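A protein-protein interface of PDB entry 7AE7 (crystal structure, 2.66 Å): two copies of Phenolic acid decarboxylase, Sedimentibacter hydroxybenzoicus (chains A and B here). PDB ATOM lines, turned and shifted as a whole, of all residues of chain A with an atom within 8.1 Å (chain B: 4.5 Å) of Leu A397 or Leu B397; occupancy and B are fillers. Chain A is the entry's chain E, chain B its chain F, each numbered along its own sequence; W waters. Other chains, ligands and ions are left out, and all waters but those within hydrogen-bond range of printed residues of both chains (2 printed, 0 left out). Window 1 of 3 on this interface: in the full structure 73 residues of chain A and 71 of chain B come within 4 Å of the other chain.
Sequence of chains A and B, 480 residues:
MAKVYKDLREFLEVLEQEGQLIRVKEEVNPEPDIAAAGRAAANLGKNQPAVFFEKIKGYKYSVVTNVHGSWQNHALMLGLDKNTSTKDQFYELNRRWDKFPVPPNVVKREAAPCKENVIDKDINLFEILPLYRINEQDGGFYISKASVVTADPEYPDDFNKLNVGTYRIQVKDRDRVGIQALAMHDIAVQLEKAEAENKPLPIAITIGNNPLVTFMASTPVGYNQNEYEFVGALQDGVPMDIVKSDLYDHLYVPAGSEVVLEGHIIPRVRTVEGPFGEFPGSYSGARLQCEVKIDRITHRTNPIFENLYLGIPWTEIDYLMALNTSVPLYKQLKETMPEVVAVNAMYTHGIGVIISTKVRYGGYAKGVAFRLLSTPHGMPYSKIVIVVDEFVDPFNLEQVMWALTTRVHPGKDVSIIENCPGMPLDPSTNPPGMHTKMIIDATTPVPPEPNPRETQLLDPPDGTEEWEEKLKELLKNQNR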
ATOM      1  N   TRP A 314     -12.762  -6.800  -0.664  1.00  0.00           N
ATOM      2  CA  TRP A 314     -11.737  -7.627  -1.297  1.00  0.00           C
ATOM      3  C   TRP A 314     -11.020  -8.550  -0.311  1.00  0.00           C
ATOM      4  O   TRP A 314     -10.707  -8.152   0.813  1.00  0.00           O
ATOM      5  CB  TRP A 314     -10.703  -6.735  -1.996  1.00  0.00           C
ATOM      6  CG  TRP A 314     -11.012  -6.425  -3.433  1.00  0.00           C
ATOM      7  CD1 TRP A 314     -12.229  -6.109  -3.962  1.00  0.00           C
ATOM      8  CD2 TRP A 314     -10.081  -6.390  -4.524  1.00  0.00           C
ATOM      9  NE1 TRP A 314     -12.116  -5.887  -5.314  1.00  0.00           N
ATOM     10  CE2 TRP A 314     -10.807  -6.054  -5.683  1.00  0.00           C
ATOM     11  CE3 TRP A 314      -8.705  -6.615  -4.632  1.00  0.00           C
ATOM     12  CZ2 TRP A 314     -10.204  -5.938  -6.935  1.00  0.00           C
ATOM     13  CZ3 TRP A 314      -8.108  -6.499  -5.875  1.00  0.00           C
ATOM     14  CH2 TRP A 314      -8.858  -6.164  -7.009  1.00  0.00           C
ATOM     15  N   ASN A 344      -9.261  -2.690 -17.123  1.00  0.00           N
ATOM     16  CA  ASN A 344      -9.332  -3.032 -15.707  1.00  0.00           C
ATOM     17  C   ASN A 344     -10.633  -3.807 -15.532  1.00  0.00           C
ATOM     18  O   ASN A 344     -11.708  -3.211 -15.427  1.00  0.00           O
ATOM     19  CB  ASN A 344      -9.268  -1.761 -14.849  1.00  0.00           C
ATOM     20  CG  ASN A 344      -9.621  -1.992 -13.379  1.00  0.00           C
ATOM     21  OD1 ASN A 344      -9.993  -3.086 -12.967  1.00  0.00           O
ATOM     22  ND2 ASN A 344      -9.493  -0.940 -12.580  1.00  0.00           N
ATOM     23  N   MET A 346     -11.189  -6.091 -12.945  1.00  0.00           N
ATOM     24  CA  MET A 346     -10.816  -6.729 -11.688  1.00  0.00           C
ATOM     25  C   MET A 346     -11.964  -6.867 -10.692  1.00  0.00           C
ATOM     26  O   MET A 346     -11.721  -7.283  -9.555  1.00  0.00           O
ATOM     27  CB  MET A 346      -9.682  -5.950 -11.014  1.00  0.00           C
ATOM     28  CG  MET A 346      -8.578  -5.453 -11.928  1.00  0.00           C
ATOM     29  SD  MET A 346      -7.039  -5.178 -11.029  1.00  0.00           S
ATOM     30  CE  MET A 346      -7.532  -3.849  -9.937  1.00  0.00           C
ATOM     31  N   TYR A 347     -13.189  -6.519 -11.064  1.00  0.00           N
ATOM     32  CA  TYR A 347     -14.276  -6.415 -10.096  1.00  0.00           C
ATOM     33  C   TYR A 347     -15.293  -7.524 -10.331  1.00  0.00           C
ATOM     34  O   TYR A 347     -16.033  -7.503 -11.321  1.00  0.00           O
ATOM     35  CB  TYR A 347     -14.902  -5.027 -10.164  1.00  0.00           C
ATOM     36  CG  TYR A 347     -13.836  -3.966 -10.096  1.00  0.00           C
ATOM     37  CD1 TYR A 347     -13.144  -3.736  -8.913  1.00  0.00           C
ATOM     38  CD2 TYR A 347     -13.487  -3.226 -11.216  1.00  0.00           C
ATOM     39  CE1 TYR A 347     -12.153  -2.785  -8.840  1.00  0.00           C
ATOM     40  CE2 TYR A 347     -12.497  -2.269 -11.153  1.00  0.00           C
ATOM     41  CZ  TYR A 347     -11.833  -2.054  -9.964  1.00  0.00           C
ATOM     42  OH  TYR A 347     -10.845  -1.103  -9.898  1.00  0.00           O
ATOM     43  N   ILE A 354     -13.382  -1.162 -16.559  1.00  0.00           N
ATOM     44  CA  ILE A 354     -12.968   0.213 -16.809  1.00  0.00           C
ATOM     45  C   ILE A 354     -11.915   0.186 -17.908  1.00  0.00           C
ATOM     46  O   ILE A 354     -10.830  -0.373 -17.719  1.00  0.00           O
ATOM     47  CB  ILE A 354     -12.415   0.885 -15.541  1.00  0.00           C
ATOM     48  CG1 ILE A 354     -13.439   0.799 -14.408  1.00  0.00           C
ATOM     49  CG2 ILE A 354     -12.046   2.332 -15.823  1.00  0.00           C
ATOM     50  CD1 ILE A 354     -12.945   1.355 -13.092  1.00  0.00           C
ATOM     51  N   ILE A 386     -17.192   1.387 -17.844  1.00  0.00           N
ATOM     52  CA  ILE A 386     -16.797   2.791 -17.796  1.00  0.00           C
ATOM     53  C   ILE A 386     -15.639   2.980 -18.763  1.00  0.00           C
ATOM     54  O   ILE A 386     -14.717   2.160 -18.792  1.00  0.00           O
ATOM     55  CB  ILE A 386     -16.395   3.218 -16.374  1.00  0.00           C
ATOM     56  CG1 ILE A 386     -17.514   2.898 -15.381  1.00  0.00           C
ATOM     57  CG2 ILE A 386     -16.047   4.698 -16.339  1.00  0.00           C
ATOM     58  CD1 ILE A 386     -17.159   3.216 -13.947  1.00  0.00           C
ATOM     59  N   VAL A 392      -5.896   8.693 -18.252  1.00  0.00           N
ATOM     60  CA  VAL A 392      -6.485   8.312 -16.975  1.00  0.00           C
ATOM     61  C   VAL A 392      -6.129   6.860 -16.692  1.00  0.00           C
ATOM     62  O   VAL A 392      -6.280   5.993 -17.561  1.00  0.00           O
ATOM     63  CB  VAL A 392      -8.009   8.520 -16.988  1.00  0.00           C
ATOM     64  CG1 VAL A 392      -8.619   8.050 -15.678  1.00  0.00           C
ATOM     65  CG2 VAL A 392      -8.345   9.982 -17.245  1.00  0.00           C
ATOM     66  N   ASP A 393      -5.646   6.596 -15.479  1.00  0.00           N
ATOM     67  CA  ASP A 393      -5.269   5.247 -15.082  1.00  0.00           C
ATOM     68  C   ASP A 393      -6.521   4.470 -14.690  1.00  0.00           C
ATOM     69  O   ASP A 393      -7.106   4.730 -13.631  1.00  0.00           O
ATOM     70  CB  ASP A 393      -4.269   5.290 -13.923  1.00  0.00           C
ATOM     71  CG  ASP A 393      -3.651   3.933 -13.623  1.00  0.00           C
ATOM     72  OD1 ASP A 393      -4.127   2.917 -14.170  1.00  0.00           O
ATOM     73  OD2 ASP A 393      -2.683   3.883 -12.837  1.00  0.00           O
ATOM     74  N   PRO A 394      -6.950   3.498 -15.503  1.00  0.00           N
ATOM     75  CA  PRO A 394      -8.190   2.768 -15.191  1.00  0.00           C
ATOM     76  C   PRO A 394      -8.107   1.949 -13.918  1.00  0.00           C
ATOM     77  O   PRO A 394      -9.153   1.530 -13.405  1.00  0.00           O
ATOM     78  CB  PRO A 394      -8.385   1.870 -16.417  1.00  0.00           C
ATOM     79  CG  PRO A 394      -7.005   1.633 -16.921  1.00  0.00           C
ATOM     80  CD  PRO A 394      -6.206   2.878 -16.614  1.00  0.00           C
ATOM     81  N   PHE A 395      -6.905   1.696 -13.409  1.00  0.00           N
ATOM     82  CA  PHE A 395      -6.714   0.989 -12.151  1.00  0.00           C
ATOM     83  C   PHE A 395      -6.704   1.917 -10.944  1.00  0.00           C
ATOM     84  O   PHE A 395      -6.782   1.432  -9.810  1.00  0.00           O
ATOM     85  CB  PHE A 395      -5.409   0.192 -12.203  1.00  0.00           C
ATOM     86  CG  PHE A 395      -5.387  -0.848 -13.279  1.00  0.00           C
ATOM     87  CD1 PHE A 395      -5.968  -2.087 -13.073  1.00  0.00           C
ATOM     88  CD2 PHE A 395      -4.805  -0.581 -14.507  1.00  0.00           C
ATOM     89  CE1 PHE A 395      -5.956  -3.046 -14.066  1.00  0.00           C
ATOM     90  CE2 PHE A 395      -4.790  -1.536 -15.505  1.00  0.00           C
ATOM     91  CZ  PHE A 395      -5.367  -2.770 -15.284  1.00  0.00           C
ATOM     92  N   ASN A 396      -6.614   3.230 -11.158  1.00  0.00           N
ATOM     93  CA  ASN A 396      -6.665   4.219 -10.082  1.00  0.00           C
ATOM     94  C   ASN A 396      -8.102   4.721  -9.995  1.00  0.00           C
ATOM     95  O   ASN A 396      -8.529   5.560 -10.793  1.00  0.00           O
ATOM     96  CB  ASN A 396      -5.684   5.357 -10.341  1.00  0.00           C
ATOM     97  CG  ASN A 396      -5.594   6.335  -9.180  1.00  0.00           C
ATOM     98  OD1 ASN A 396      -6.573   6.584  -8.473  1.00  0.00           O
ATOM     99  ND2 ASN A 396      -4.407   6.896  -8.976  1.00  0.00           N
ATOM    100  N   LEU A 397      -8.846   4.213  -9.010  1.00  0.00           N
ATOM    101  CA  LEU A 397     -10.263   4.539  -8.908  1.00  0.00           C
ATOM    102  C   LEU A 397     -10.504   5.987  -8.500  1.00  0.00           C
ATOM    103  O   LEU A 397     -11.590   6.513  -8.759  1.00  0.00           O
ATOM    104  CB  LEU A 397     -10.947   3.583  -7.931  1.00  0.00           C
ATOM    105  CG  LEU A 397     -10.933   2.123  -8.391  1.00  0.00           C
ATOM    106  CD1 LEU A 397     -11.855   1.255  -7.548  1.00  0.00           C
ATOM    107  CD2 LEU A 397     -11.316   2.043  -9.858  1.00  0.00           C
ATOM    108  N   GLU A 398      -9.528   6.645  -7.869  1.00  0.00           N
ATOM    109  CA  GLU A 398      -9.658   8.078  -7.622  1.00  0.00           C
ATOM    110  C   GLU A 398      -9.656   8.863  -8.930  1.00  0.00           C
ATOM    111  O   GLU A 398     -10.477   9.771  -9.124  1.00  0.00           O
ATOM    112  CB  GLU A 398      -8.533   8.561  -6.702  1.00  0.00           C
ATOM    113  CG  GLU A 398      -8.703   8.177  -5.239  1.00  0.00           C
ATOM    114  CD  GLU A 398      -8.302   6.740  -4.955  1.00  0.00           C
ATOM    115  OE1 GLU A 398      -7.149   6.374  -5.270  1.00  0.00           O
ATOM    116  OE2 GLU A 398      -9.135   5.981  -4.411  1.00  0.00           O
ATOM    117  N   GLN A 399      -8.753   8.512  -9.849  1.00  0.00           N
ATOM    118  CA  GLN A 399      -8.741   9.148 -11.162  1.00  0.00           C
ATOM    119  C   GLN A 399     -10.017   8.837 -11.933  1.00  0.00           C
ATOM    120  O   GLN A 399     -10.541   9.694 -12.655  1.00  0.00           O
ATOM    121  CB  GLN A 399      -7.512   8.696 -11.952  1.00  0.00           C
ATOM    122  CG  GLN A 399      -6.302   9.604 -11.808  1.00  0.00           C
ATOM    123  CD  GLN A 399      -5.096   9.088 -12.570  1.00  0.00           C
ATOM    124  OE1 GLN A 399      -5.166   8.848 -13.775  1.00  0.00           O
ATOM    125  NE2 GLN A 399      -3.982   8.912 -11.868  1.00  0.00           N
ATOM    126  N   VAL A 400     -10.533   7.614 -11.792  1.00  0.00           N
ATOM    127  CA  VAL A 400     -11.782   7.251 -12.458  1.00  0.00           C
ATOM    128  C   VAL A 400     -12.945   8.052 -11.889  1.00  0.00           C
ATOM    129  O   VAL A 400     -13.849   8.469 -12.624  1.00  0.00           O
ATOM    130  CB  VAL A 400     -12.025   5.735 -12.345  1.00  0.00           C
ATOM    131  CG1 VAL A 400     -13.366   5.363 -12.955  1.00  0.00           C
ATOM    132  CG2 VAL A 400     -10.898   4.968 -13.020  1.00  0.00           C
ATOM    133  N   MET A 401     -12.950   8.274 -10.573  1.00  0.00           N
ATOM    134  CA  MET A 401     -13.973   9.123  -9.971  1.00  0.00           C
ATOM    135  C   MET A 401     -13.871  10.549 -10.496  1.00  0.00           C
ATOM    136  O   MET A 401     -14.891  11.197 -10.764  1.00  0.00           O
ATOM    137  CB  MET A 401     -13.848   9.094  -8.448  1.00  0.00           C
ATOM    138  CG  MET A 401     -14.729   8.057  -7.766  1.00  0.00           C
ATOM    139  SD  MET A 401     -16.486   8.404  -7.947  1.00  0.00           S
ATOM    140  CE  MET A 401     -17.114   6.748  -8.186  1.00  0.00           C
ATOM    141  N   TRP A 402     -12.644  11.053 -10.659  1.00  0.00           N
ATOM    142  CA  TRP A 402     -12.468  12.365 -11.277  1.00  0.00           C
ATOM    143  C   TRP A 402     -13.054  12.393 -12.686  1.00  0.00           C
ATOM    144  O   TRP A 402     -13.743  13.351 -13.066  1.00  0.00           O
ATOM    145  CB  TRP A 402     -10.987  12.735 -11.316  1.00  0.00           C
ATOM    146  CG  TRP A 402     -10.709  13.949 -12.143  1.00  0.00           C
ATOM    147  CD1 TRP A 402     -11.002  15.241 -11.821  1.00  0.00           C
ATOM    148  CD2 TRP A 402     -10.104  13.987 -13.441  1.00  0.00           C
ATOM    149  NE1 TRP A 402     -10.606  16.084 -12.831  1.00  0.00           N
ATOM    150  CE2 TRP A 402     -10.052  15.338 -13.838  1.00  0.00           C
ATOM    151  CE3 TRP A 402      -9.596  13.010 -14.304  1.00  0.00           C
ATOM    152  CZ2 TRP A 402      -9.512  15.738 -15.058  1.00  0.00           C
ATOM    153  CZ3 TRP A 402      -9.060  13.410 -15.516  1.00  0.00           C
ATOM    154  CH2 TRP A 402      -9.023  14.762 -15.881  1.00  0.00           C
ATOM    155  N   ALA A 403     -12.782  11.350 -13.474  1.00  0.00           N
ATOM    156  CA  ALA A 403     -13.304  11.286 -14.835  1.00  0.00           C
ATOM    157  C   ALA A 403     -14.825  11.272 -14.840  1.00  0.00           C
ATOM    158  O   ALA A 403     -15.456  11.971 -15.641  1.00  0.00           O
ATOM    159  CB  ALA A 403     -12.752  10.056 -15.554  1.00  0.00           C
ATOM    160  N   LEU A 404     -15.434  10.492 -13.943  1.00  0.00           N
ATOM    161  CA  LEU A 404     -16.892  10.452 -13.864  1.00  0.00           C
ATOM    162  C   LEU A 404     -17.464  11.809 -13.477  1.00  0.00           C
ATOM    163  O   LEU A 404     -18.470  12.252 -14.044  1.00  0.00           O
ATOM    164  CB  LEU A 404     -17.346   9.387 -12.866  1.00  0.00           C
ATOM    165  CG  LEU A 404     -17.018   7.922 -13.153  1.00  0.00           C
ATOM    166  CD1 LEU A 404     -17.397   7.060 -11.958  1.00  0.00           C
ATOM    167  CD2 LEU A 404     -17.727   7.448 -14.407  1.00  0.00           C
ATOM    168  N   TYR B 347     -14.854  13.546  -3.800  1.00  0.00           N
ATOM    169  CA  TYR B 347     -14.526  13.510  -5.220  1.00  0.00           C
ATOM    170  C   TYR B 347     -14.956  14.813  -5.882  1.00  0.00           C
ATOM    171  O   TYR B 347     -16.148  15.040  -6.111  1.00  0.00           O
ATOM    172  CB  TYR B 347     -15.161  12.282  -5.863  1.00  0.00           C
ATOM    173  CG  TYR B 347     -14.749  11.041  -5.114  1.00  0.00           C
ATOM    174  CD1 TYR B 347     -13.425  10.619  -5.121  1.00  0.00           C
ATOM    175  CD2 TYR B 347     -15.661  10.322  -4.354  1.00  0.00           C
ATOM    176  CE1 TYR B 347     -13.026   9.503  -4.423  1.00  0.00           C
ATOM    177  CE2 TYR B 347     -15.271   9.197  -3.652  1.00  0.00           C
ATOM    178  CZ  TYR B 347     -13.951   8.795  -3.690  1.00  0.00           C
ATOM    179  OH  TYR B 347     -13.551   7.680  -2.993  1.00  0.00           O
ATOM    180  N   ILE B 354     -20.703   9.090  -2.138  1.00  0.00           N
ATOM    181  CA  ILE B 354     -21.048   7.709  -1.813  1.00  0.00           C
ATOM    182  C   ILE B 354     -21.530   7.685  -0.368  1.00  0.00           C
ATOM    183  O   ILE B 354     -20.755   7.953   0.557  1.00  0.00           O
ATOM    184  CB  ILE B 354     -19.858   6.758  -2.008  1.00  0.00           C
ATOM    185  CG1 ILE B 354     -19.245   6.941  -3.397  1.00  0.00           C
ATOM    186  CG2 ILE B 354     -20.289   5.316  -1.795  1.00  0.00           C
ATOM    187  CD1 ILE B 354     -17.962   6.165  -3.604  1.00  0.00           C
ATOM    188  N   PRO B 394     -17.780   3.193   2.489  1.00  0.00           N
ATOM    189  CA  PRO B 394     -17.889   4.078   1.319  1.00  0.00           C
ATOM    190  C   PRO B 394     -16.578   4.735   0.932  1.00  0.00           C
ATOM    191  O   PRO B 394     -16.504   5.345  -0.143  1.00  0.00           O
ATOM    192  CB  PRO B 394     -18.927   5.116   1.758  1.00  0.00           C
ATOM    193  CG  PRO B 394     -18.795   5.170   3.239  1.00  0.00           C
ATOM    194  CD  PRO B 394     -18.336   3.808   3.706  1.00  0.00           C
ATOM    195  N   PHE B 395     -15.553   4.642   1.774  1.00  0.00           N
ATOM    196  CA  PHE B 395     -14.227   5.146   1.455  1.00  0.00           C
ATOM    197  C   PHE B 395     -13.333   4.089   0.820  1.00  0.00           C
ATOM    198  O   PHE B 395     -12.218   4.415   0.397  1.00  0.00           O
ATOM    199  CB  PHE B 395     -13.570   5.695   2.724  1.00  0.00           C
ATOM    200  CG  PHE B 395     -14.316   6.849   3.335  1.00  0.00           C
ATOM    201  CD1 PHE B 395     -14.203   8.119   2.801  1.00  0.00           C
ATOM    202  CD2 PHE B 395     -15.148   6.658   4.426  1.00  0.00           C
ATOM    203  CE1 PHE B 395     -14.888   9.184   3.354  1.00  0.00           C
ATOM    204  CE2 PHE B 395     -15.840   7.717   4.981  1.00  0.00           C
ATOM    205  CZ  PHE B 395     -15.710   8.982   4.445  1.00  0.00           C
ATOM    206  N   ASN B 396     -13.797   2.841   0.743  1.00  0.00           N
ATOM    207  CA  ASN B 396     -13.061   1.739   0.123  1.00  0.00           C
ATOM    208  C   ASN B 396     -13.675   1.512  -1.254  1.00  0.00           C
ATOM    209  O   ASN B 396     -14.709   0.853  -1.384  1.00  0.00           O
ATOM    210  CB  ASN B 396     -13.132   0.486   0.993  1.00  0.00           C
ATOM    211  CG  ASN B 396     -12.322  -0.677   0.433  1.00  0.00           C
ATOM    212  OD1 ASN B 396     -12.266  -0.899  -0.778  1.00  0.00           O
ATOM    213  ND2 ASN B 396     -11.688  -1.427   1.324  1.00  0.00           N
ATOM    214  N   LEU B 397     -13.027   2.053  -2.286  1.00  0.00           N
ATOM    215  CA  LEU B 397     -13.625   2.042  -3.618  1.00  0.00           C
ATOM    216  C   LEU B 397     -13.723   0.634  -4.197  1.00  0.00           C
ATOM    217  O   LEU B 397     -14.621   0.365  -5.003  1.00  0.00           O
ATOM    218  CB  LEU B 397     -12.844   2.974  -4.544  1.00  0.00           C
ATOM    219  CG  LEU B 397     -13.060   4.458  -4.222  1.00  0.00           C
ATOM    220  CD1 LEU B 397     -12.564   5.370  -5.333  1.00  0.00           C
ATOM    221  CD2 LEU B 397     -14.530   4.725  -3.938  1.00  0.00           C
ATOM    222  N   GLU B 398     -12.825  -0.276  -3.807  1.00  0.00           N
ATOM    223  CA  GLU B 398     -12.964  -1.671  -4.225  1.00  0.00           C
ATOM    224  C   GLU B 398     -14.284  -2.253  -3.730  1.00  0.00           C
ATOM    225  O   GLU B 398     -15.008  -2.929  -4.476  1.00  0.00           O
ATOM    226  CB  GLU B 398     -11.791  -2.502  -3.700  1.00  0.00           C
ATOM    227  CG  GLU B 398     -10.401  -1.968  -4.019  1.00  0.00           C
ATOM    228  CD  GLU B 398      -9.304  -2.834  -3.415  1.00  0.00           C
ATOM    229  OE1 GLU B 398      -9.360  -3.097  -2.193  1.00  0.00           O
ATOM    230  OE2 GLU B 398      -8.393  -3.260  -4.160  1.00  0.00           O
ATOM    231  N   GLN B 399     -14.615  -1.991  -2.464  1.00  0.00           N
ATOM    232  CA  GLN B 399     -15.866  -2.483  -1.897  1.00  0.00           C
ATOM    233  C   GLN B 399     -17.071  -1.862  -2.589  1.00  0.00           C
ATOM    234  O   GLN B 399     -18.086  -2.534  -2.812  1.00  0.00           O
ATOM    235  CB  GLN B 399     -15.909  -2.184  -0.401  1.00  0.00           C
ATOM    236  CG  GLN B 399     -15.575  -3.364   0.478  1.00  0.00           C
ATOM    237  CD  GLN B 399     -15.769  -3.053   1.945  1.00  0.00           C
ATOM    238  OE1 GLN B 399     -16.898  -2.922   2.417  1.00  0.00           O
ATOM    239  NE2 GLN B 399     -14.667  -2.926   2.676  1.00  0.00           N
ATOM    240  N   VAL B 400     -16.989  -0.569  -2.912  1.00  0.00           N
ATOM    241  CA  VAL B 400     -18.091   0.088  -3.605  1.00  0.00           C
ATOM    242  C   VAL B 400     -18.268  -0.505  -4.995  1.00  0.00           C
ATOM    243  O   VAL B 400     -19.394  -0.650  -5.485  1.00  0.00           O
ATOM    244  CB  VAL B 400     -17.865   1.609  -3.658  1.00  0.00           C
ATOM    245  CG1 VAL B 400     -19.102   2.303  -4.190  1.00  0.00           C
ATOM    246  CG2 VAL B 400     -17.516   2.138  -2.277  1.00  0.00           C
ATOM    247  N   MET B 401     -17.161  -0.861  -5.650  1.00  0.00           N
ATOM    248  CA  MET B 401     -17.259  -1.554  -6.932  1.00  0.00           C
ATOM    249  C   MET B 401     -17.934  -2.910  -6.767  1.00  0.00           C
ATOM    250  O   MET B 401     -18.737  -3.316  -7.615  1.00  0.00           O
ATOM    251  CB  MET B 401     -15.873  -1.715  -7.554  1.00  0.00           C
ATOM    252  CG  MET B 401     -15.369  -0.479  -8.287  1.00  0.00           C
ATOM    253  SD  MET B 401     -16.407   0.022  -9.677  1.00  0.00           S
ATOM    254  CE  MET B 401     -16.570  -1.521 -10.575  1.00  0.00           C
HETATM  255  O   HOH W   1     -11.289  -4.198  -0.101  1.00  0.00           O
HETATM  256  O   HOH W   2     -11.132   7.306  -2.673  1.00  0.00           O
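The backbone NH of Glu A398 sits at hydrogen-bond distance from the side-chain amide oxygen of Asn A396, at 3.0 Å.
OD1 of Asn B396 is in hydrogen-bond range of N of Glu B398.
The side-chain amide nitrogen (ND2) of Asn A344 sits at hydrogen-bond distance from the side-chain hydroxyl (OH) of Tyr A347 (3.0 Å).
Among the printed residues, merely in contact across the chains: Trp A314 with Glu B398 (3.4 Å), Tyr A347 with Met B401 (3.6 Å), Leu A397 with Leu B397 (3.5 Å), Leu A397 with Met B401 (3.99 Å), Glu A398 with Leu B397 (3.6 Å) and Met A401 with Tyr B347 (3.7 Å).
Printed residues of chain B within 4 Å of Leu A397: Leu B397 (3.5 Å) and Met B401 (3.99 Å).
Leu B397 touches two residues of chain A.
Of the printed residues of chain A, Tyr B347 touches Met A401 (3.7 Å).
Of the printed residues of chain B, Trp A314 touches Glu B398 (3.4 Å).
Of the printed residues of chain B, Glu A398 touches Leu B397.
Asn B396 touches none of the printed residues of chain A.
Gln B399 touches none of the printed residues of chain A.
The nearest residue of chain A that does not touch Leu B397 is Met A401 (4.2 Å).
Hydrophobic or aromatic side chains of chain A within 4 Å of the printed part of chain B: Trp A314, Tyr A347, Leu A397 and Met A401.
Tyr A347 touches Met B401, and with the chains exchanged Met A401 touches Tyr B347.
Leu A397 touches its own counterpart, Leu B397.
Leu A397 touches Met B401, but with the chains exchanged Met A401 does not touch Leu B397 (4.2 Å).
Glu A398 touches Leu B397, but with the chains exchanged Leu A397 does not touch Glu B398 (4.2 Å).
Water W2 lies within hydrogen-bond range of the side-chain hydroxyl (OH) of Tyr B347 and the side-chain carboxylate (OE2) of Glu A398.
Water W1 lies within hydrogen-bond range of the backbone NH (N) of Trp A314, the side-chain carboxylate (OE1) of Glu B398 and the side-chain amide nitrogen (ND2) of Asn B396.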
